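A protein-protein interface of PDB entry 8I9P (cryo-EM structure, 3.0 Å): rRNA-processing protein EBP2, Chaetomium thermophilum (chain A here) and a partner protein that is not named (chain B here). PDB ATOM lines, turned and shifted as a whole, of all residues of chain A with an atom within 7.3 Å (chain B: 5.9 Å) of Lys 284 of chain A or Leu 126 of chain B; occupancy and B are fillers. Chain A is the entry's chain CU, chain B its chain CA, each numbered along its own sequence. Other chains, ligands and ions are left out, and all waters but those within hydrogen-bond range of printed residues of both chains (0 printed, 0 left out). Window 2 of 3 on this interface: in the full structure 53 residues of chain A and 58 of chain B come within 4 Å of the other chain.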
ATOM      1  N   ARG A 277     -17.200 -13.997 -27.573  1.00  0.00           N
ATOM      2  CA  ARG A 277     -17.193 -15.440 -27.447  1.00  0.00           C
ATOM      3  C   ARG A 277     -17.566 -16.009 -28.804  1.00  0.00           C
ATOM      4  O   ARG A 277     -18.184 -15.329 -29.625  1.00  0.00           O
ATOM      5  CB  ARG A 277     -18.131 -15.889 -26.321  1.00  0.00           C
ATOM      6  CG  ARG A 277     -19.123 -14.798 -25.936  1.00  0.00           C
ATOM      7  CD  ARG A 277     -20.274 -15.239 -25.034  1.00  0.00           C
ATOM      8  NE  ARG A 277     -20.830 -14.112 -24.288  1.00  0.00           N
ATOM      9  CZ  ARG A 277     -21.758 -14.224 -23.345  1.00  0.00           C
ATOM     10  NH1 ARG A 277     -22.279 -15.398 -23.026  1.00  0.00           N
ATOM     11  NH2 ARG A 277     -22.159 -13.137 -22.692  1.00  0.00           N
ATOM     12  N   THR A 278     -17.135 -17.234 -29.064  1.00  0.00           N
ATOM     13  CA  THR A 278     -17.260 -17.763 -30.409  1.00  0.00           C
ATOM     14  C   THR A 278     -18.729 -17.939 -30.781  1.00  0.00           C
ATOM     15  O   THR A 278     -19.603 -18.071 -29.922  1.00  0.00           O
ATOM     16  CB  THR A 278     -16.542 -19.101 -30.528  1.00  0.00           C
ATOM     17  OG1 THR A 278     -17.100 -20.032 -29.590  1.00  0.00           O
ATOM     18  CG2 THR A 278     -15.073 -18.907 -30.210  1.00  0.00           C
ATOM     19  N   ASP A 279     -18.992 -17.943 -32.091  1.00  0.00           N
ATOM     20  CA  ASP A 279     -20.360 -18.065 -32.574  1.00  0.00           C
ATOM     21  C   ASP A 279     -20.970 -19.422 -32.248  1.00  0.00           C
ATOM     22  O   ASP A 279     -22.193 -19.576 -32.337  1.00  0.00           O
ATOM     23  CB  ASP A 279     -20.397 -17.791 -34.075  1.00  0.00           C
ATOM     24  CG  ASP A 279     -20.576 -16.321 -34.377  1.00  0.00           C
ATOM     25  OD1 ASP A 279     -20.463 -15.506 -33.436  1.00  0.00           O
ATOM     26  OD2 ASP A 279     -20.817 -15.977 -35.553  1.00  0.00           O
ATOM     27  N   ALA A 280     -20.148 -20.397 -31.852  1.00  0.00           N
ATOM     28  CA  ALA A 280     -20.668 -21.606 -31.223  1.00  0.00           C
ATOM     29  C   ALA A 280     -21.373 -21.287 -29.906  1.00  0.00           C
ATOM     30  O   ALA A 280     -22.419 -21.872 -29.604  1.00  0.00           O
ATOM     31  CB  ALA A 280     -19.539 -22.609 -31.000  1.00  0.00           C
ATOM     32  N   THR A 281     -20.813 -20.369 -29.105  1.00  0.00           N
ATOM     33  CA  THR A 281     -21.435 -20.024 -27.826  1.00  0.00           C
ATOM     34  C   THR A 281     -22.784 -19.346 -28.038  1.00  0.00           C
ATOM     35  O   THR A 281     -23.755 -19.637 -27.331  1.00  0.00           O
ATOM     36  CB  THR A 281     -20.508 -19.127 -26.998  1.00  0.00           C
ATOM     37  OG1 THR A 281     -19.270 -19.806 -26.771  1.00  0.00           O
ATOM     38  CG2 THR A 281     -21.135 -18.807 -25.636  1.00  0.00           C
ATOM     39  N   MET A 282     -22.873 -18.455 -29.028  1.00  0.00           N
ATOM     40  CA  MET A 282     -24.157 -17.820 -29.302  1.00  0.00           C
ATOM     41  C   MET A 282     -25.125 -18.771 -29.982  1.00  0.00           C
ATOM     42  O   MET A 282     -26.340 -18.641 -29.810  1.00  0.00           O
ATOM     43  CB  MET A 282     -23.974 -16.547 -30.114  1.00  0.00           C
ATOM     44  CG  MET A 282     -22.929 -15.675 -29.510  1.00  0.00           C
ATOM     45  SD  MET A 282     -23.552 -15.351 -27.854  1.00  0.00           S
ATOM     46  CE  MET A 282     -23.103 -13.658 -27.655  1.00  0.00           C
ATOM     47  N   GLU A 283     -24.609 -19.740 -30.737  1.00  0.00           N
ATOM     48  CA  GLU A 283     -25.459 -20.825 -31.206  1.00  0.00           C
ATOM     49  C   GLU A 283     -26.063 -21.583 -30.029  1.00  0.00           C
ATOM     50  O   GLU A 283     -27.256 -21.898 -30.032  1.00  0.00           O
ATOM     51  CB  GLU A 283     -24.650 -21.757 -32.111  1.00  0.00           C
ATOM     52  CG  GLU A 283     -25.248 -23.140 -32.320  1.00  0.00           C
ATOM     53  CD  GLU A 283     -26.604 -23.125 -33.015  1.00  0.00           C
ATOM     54  OE1 GLU A 283     -26.920 -22.154 -33.737  1.00  0.00           O
ATOM     55  OE2 GLU A 283     -27.368 -24.094 -32.830  1.00  0.00           O
ATOM     56  N   LYS A 284     -25.259 -21.823 -28.986  1.00  0.00           N
ATOM     57  CA  LYS A 284     -25.739 -22.501 -27.780  1.00  0.00           C
ATOM     58  C   LYS A 284     -26.767 -21.660 -27.022  1.00  0.00           C
ATOM     59  O   LYS A 284     -27.748 -22.200 -26.488  1.00  0.00           O
ATOM     60  CB  LYS A 284     -24.553 -22.847 -26.876  1.00  0.00           C
ATOM     61  CG  LYS A 284     -23.680 -23.994 -27.382  1.00  0.00           C
ATOM     62  CD  LYS A 284     -23.287 -24.952 -26.269  1.00  0.00           C
ATOM     63  CE  LYS A 284     -21.864 -25.441 -26.462  1.00  0.00           C
ATOM     64  NZ  LYS A 284     -21.459 -25.425 -27.896  1.00  0.00           N
ATOM     65  N   VAL A 285     -26.555 -20.342 -26.932  1.00  0.00           N
ATOM     66  CA  VAL A 285     -27.508 -19.535 -26.167  1.00  0.00           C
ATOM     67  C   VAL A 285     -28.820 -19.338 -26.947  1.00  0.00           C
ATOM     68  O   VAL A 285     -29.905 -19.436 -26.353  1.00  0.00           O
ATOM     69  CB  VAL A 285     -26.876 -18.210 -25.666  1.00  0.00           C
ATOM     70  CG1 VAL A 285     -25.572 -18.474 -24.927  1.00  0.00           C
ATOM     71  CG2 VAL A 285     -26.625 -17.216 -26.765  1.00  0.00           C
ATOM     72  N   LYS A 286     -28.762 -19.129 -28.280  1.00  0.00           N
ATOM     73  CA  LYS A 286     -29.955 -19.290 -29.121  1.00  0.00           C
ATOM     74  C   LYS A 286     -30.606 -20.656 -28.936  1.00  0.00           C
ATOM     75  O   LYS A 286     -31.837 -20.765 -28.956  1.00  0.00           O
ATOM     76  CB  LYS A 286     -29.641 -19.077 -30.617  1.00  0.00           C
ATOM     77  CG  LYS A 286     -29.060 -17.743 -31.222  1.00  0.00           C
ATOM     78  CD  LYS A 286     -29.505 -16.394 -30.605  1.00  0.00           C
ATOM     79  CE  LYS A 286     -28.770 -15.949 -29.363  1.00  0.00           C
ATOM     80  NZ  LYS A 286     -28.988 -14.500 -29.116  1.00  0.00           N
ATOM     81  N   GLN A 287     -29.800 -21.704 -28.752  1.00  0.00           N
ATOM     82  CA  GLN A 287     -30.359 -23.042 -28.636  1.00  0.00           C
ATOM     83  C   GLN A 287     -31.149 -23.180 -27.344  1.00  0.00           C
ATOM     84  O   GLN A 287     -32.246 -23.749 -27.346  1.00  0.00           O
ATOM     85  CB  GLN A 287     -29.232 -24.077 -28.757  1.00  0.00           C
ATOM     86  CG  GLN A 287     -29.626 -25.564 -28.967  1.00  0.00           C
ATOM     87  CD  GLN A 287     -30.225 -26.290 -27.763  1.00  0.00           C
ATOM     88  OE1 GLN A 287     -30.105 -25.848 -26.620  1.00  0.00           O
ATOM     89  NE2 GLN A 287     -30.858 -27.428 -28.026  1.00  0.00           N
ATOM     90  N   LYS A 288     -30.640 -22.633 -26.233  1.00  0.00           N
ATOM     91  CA  LYS A 288     -31.431 -22.725 -25.007  1.00  0.00           C
ATOM     92  C   LYS A 288     -32.652 -21.813 -25.055  1.00  0.00           C
ATOM     93  O   LYS A 288     -33.690 -22.157 -24.482  1.00  0.00           O
ATOM     94  CB  LYS A 288     -30.652 -22.410 -23.730  1.00  0.00           C
ATOM     95  CG  LYS A 288     -30.057 -21.030 -23.575  1.00  0.00           C
ATOM     96  CD  LYS A 288     -29.644 -20.773 -22.104  1.00  0.00           C
ATOM     97  CE  LYS A 288     -29.081 -21.989 -21.399  1.00  0.00           C
ATOM     98  NZ  LYS A 288     -28.132 -21.662 -20.289  1.00  0.00           N
ATOM     99  N   LEU A 289     -32.548 -20.634 -25.692  1.00  0.00           N
ATOM    100  CA  LEU A 289     -33.728 -19.772 -25.794  1.00  0.00           C
ATOM    101  C   LEU A 289     -34.830 -20.424 -26.621  1.00  0.00           C
ATOM    102  O   LEU A 289     -35.998 -20.426 -26.208  1.00  0.00           O
ATOM    103  CB  LEU A 289     -33.372 -18.401 -26.372  1.00  0.00           C
ATOM    104  CG  LEU A 289     -32.415 -17.542 -25.539  1.00  0.00           C
ATOM    105  CD1 LEU A 289     -31.604 -16.561 -26.387  1.00  0.00           C
ATOM    106  CD2 LEU A 289     -33.160 -16.807 -24.424  1.00  0.00           C
ATOM    107  N   ILE A 290     -34.485 -21.014 -27.770  1.00  0.00           N
ATOM    108  CA  ILE A 290     -35.506 -21.701 -28.560  1.00  0.00           C
ATOM    109  C   ILE A 290     -36.008 -22.935 -27.818  1.00  0.00           C
ATOM    110  O   ILE A 290     -37.194 -23.271 -27.892  1.00  0.00           O
ATOM    111  CB  ILE A 290     -34.996 -22.010 -29.991  1.00  0.00           C
ATOM    112  CG1 ILE A 290     -33.839 -23.030 -30.065  1.00  0.00           C
ATOM    113  CG2 ILE A 290     -34.627 -20.713 -30.716  1.00  0.00           C
ATOM    114  CD1 ILE A 290     -34.217 -24.527 -30.152  1.00  0.00           C
ATOM    115  N   MET B 123     -17.256 -15.657 -18.772  1.00  0.00           N
ATOM    116  CA  MET B 123     -18.004 -15.367 -19.989  1.00  0.00           C
ATOM    117  C   MET B 123     -18.544 -16.636 -20.631  1.00  0.00           C
ATOM    118  O   MET B 123     -19.499 -16.575 -21.413  1.00  0.00           O
ATOM    119  CB  MET B 123     -17.097 -14.627 -20.968  1.00  0.00           C
ATOM    120  CG  MET B 123     -16.955 -13.143 -20.684  1.00  0.00           C
ATOM    121  SD  MET B 123     -15.918 -12.320 -21.900  1.00  0.00           S
ATOM    122  CE  MET B 123     -15.949 -10.630 -21.321  1.00  0.00           C
ATOM    123  N   GLU B 124     -17.936 -17.788 -20.326  1.00  0.00           N
ATOM    124  CA  GLU B 124     -18.382 -19.065 -20.871  1.00  0.00           C
ATOM    125  C   GLU B 124     -19.724 -19.480 -20.279  1.00  0.00           C
ATOM    126  O   GLU B 124     -20.433 -20.288 -20.884  1.00  0.00           O
ATOM    127  CB  GLU B 124     -17.313 -20.136 -20.611  1.00  0.00           C
ATOM    128  CG  GLU B 124     -17.482 -21.533 -21.263  1.00  0.00           C
ATOM    129  CD  GLU B 124     -18.306 -21.553 -22.552  1.00  0.00           C
ATOM    130  OE1 GLU B 124     -17.894 -20.914 -23.542  1.00  0.00           O
ATOM    131  OE2 GLU B 124     -19.363 -22.223 -22.580  1.00  0.00           O
ATOM    132  N   GLU B 125     -20.094 -18.926 -19.126  1.00  0.00           N
ATOM    133  CA  GLU B 125     -21.408 -19.185 -18.558  1.00  0.00           C
ATOM    134  C   GLU B 125     -22.514 -18.703 -19.490  1.00  0.00           C
ATOM    135  O   GLU B 125     -22.463 -17.596 -20.034  1.00  0.00           O
ATOM    136  CB  GLU B 125     -21.517 -18.530 -17.178  1.00  0.00           C
ATOM    137  CG  GLU B 125     -20.826 -19.310 -16.048  1.00  0.00           C
ATOM    138  CD  GLU B 125     -19.318 -19.127 -15.970  1.00  0.00           C
ATOM    139  OE1 GLU B 125     -18.631 -19.200 -17.006  1.00  0.00           O
ATOM    140  OE2 GLU B 125     -18.800 -18.936 -14.858  1.00  0.00           O
ATOM    141  N   LEU B 126     -23.508 -19.565 -19.671  1.00  0.00           N
ATOM    142  CA  LEU B 126     -24.326 -19.631 -20.870  1.00  0.00           C
ATOM    143  C   LEU B 126     -25.675 -18.942 -20.693  1.00  0.00           C
ATOM    144  O   LEU B 126     -26.550 -19.073 -21.549  1.00  0.00           O
ATOM    145  CB  LEU B 126     -24.455 -21.115 -21.270  1.00  0.00           C
ATOM    146  CG  LEU B 126     -24.607 -21.745 -22.666  1.00  0.00           C
ATOM    147  CD1 LEU B 126     -24.235 -23.211 -22.582  1.00  0.00           C
ATOM    148  CD2 LEU B 126     -26.005 -21.664 -23.247  1.00  0.00           C
ATOM    149  N   HIS B 127     -25.842 -18.183 -19.610  1.00  0.00           N
ATOM    150  CA  HIS B 127     -27.109 -17.562 -19.254  1.00  0.00           C
ATOM    151  C   HIS B 127     -27.115 -16.040 -19.409  1.00  0.00           C
ATOM    152  O   HIS B 127     -28.130 -15.398 -19.121  1.00  0.00           O
ATOM    153  CB  HIS B 127     -27.467 -17.969 -17.826  1.00  0.00           C
ATOM    154  CG  HIS B 127     -26.995 -16.998 -16.787  1.00  0.00           C
ATOM    155  ND1 HIS B 127     -25.664 -16.682 -16.627  1.00  0.00           N
ATOM    156  CD2 HIS B 127     -27.666 -16.277 -15.859  1.00  0.00           C
ATOM    157  CE1 HIS B 127     -25.536 -15.807 -15.648  1.00  0.00           C
ATOM    158  NE2 HIS B 127     -26.735 -15.544 -15.166  1.00  0.00           N
ATOM    159  N   PHE B 128     -26.026 -15.449 -19.905  1.00  0.00           N
ATOM    160  CA  PHE B 128     -25.869 -13.996 -19.879  1.00  0.00           C
ATOM    161  C   PHE B 128     -26.573 -13.286 -21.032  1.00  0.00           C
ATOM    162  O   PHE B 128     -27.102 -12.184 -20.836  1.00  0.00           O
ATOM    163  CB  PHE B 128     -24.389 -13.620 -19.893  1.00  0.00           C
ATOM    164  CG  PHE B 128     -23.697 -13.819 -18.575  1.00  0.00           C
ATOM    165  CD1 PHE B 128     -23.915 -12.953 -17.514  1.00  0.00           C
ATOM    166  CD2 PHE B 128     -22.801 -14.858 -18.408  1.00  0.00           C
ATOM    167  CE1 PHE B 128     -23.263 -13.144 -16.302  1.00  0.00           C
ATOM    168  CE2 PHE B 128     -22.149 -15.047 -17.205  1.00  0.00           C
ATOM    169  CZ  PHE B 128     -22.379 -14.190 -16.152  1.00  0.00           C
ATOM    170  N   GLN B 129     -26.529 -13.863 -22.237  1.00  0.00           N
ATOM    171  CA  GLN B 129     -27.281 -13.420 -23.413  1.00  0.00           C
ATOM    172  C   GLN B 129     -26.869 -12.031 -23.922  1.00  0.00           C
ATOM    173  O   GLN B 129     -27.647 -11.374 -24.618  1.00  0.00           O
ATOM    174  CB  GLN B 129     -28.797 -13.460 -23.152  1.00  0.00           C
ATOM    175  CG  GLN B 129     -29.665 -13.944 -24.310  1.00  0.00           C
ATOM    176  CD  GLN B 129     -31.155 -13.813 -24.025  1.00  0.00           C
ATOM    177  OE1 GLN B 129     -31.631 -14.199 -22.955  1.00  0.00           O
ATOM    178  NE2 GLN B 129     -31.895 -13.266 -24.980  1.00  0.00           N
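Among the printed residues, merely in contact across the chains: Leu 289 of chain A with Gln 129 of chain B, Val 285 of chain A with Leu 126 of chain B, Arg 277 of chain A with Phe 128 of chain B, Thr 281 of chain A with Glu 124 of chain B, Arg 277 of chain A with Glu 125 of chain B and Lys 284 of chain A with Leu 126 of chain B.
Lys 284 of chain A touches one residue of chain B. Of the printed residues of chain B, Val 285 of chain A touches Leu 126. Printed residues of chain A within 4 Å of Glu 124 of chain B: Thr 281 (3.7 Å). Of the printed residues of chain A, Glu 125 of chain B touches Arg 277 (3.7 Å). Printed residues of chain A within 4 Å of Leu 126 of chain B: Lys 284, Val 285 and Lys 288. Of the printed residues of chain A, Gln 129 of chain B touches Leu 289.
The guanidinium group (NH1) of Arg 277 of chain A lies within hydrogen-bond range of the backbone carbonyl oxygen (O) of Met 123 of chain B. The side-chain amino group of Lys 288 of chain A is in hydrogen-bond range of the backbone carbonyl oxygen of Leu 126 of chain B.
Hydrophobic or aromatic side chains of chain A within 4 Å of the printed part of chain B: Val 285 and Leu 289. Among the printed residues, no Asp or Glu carboxylate lies within 4 Å of a Lys or Arg side-chain nitrogen of the other chain.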
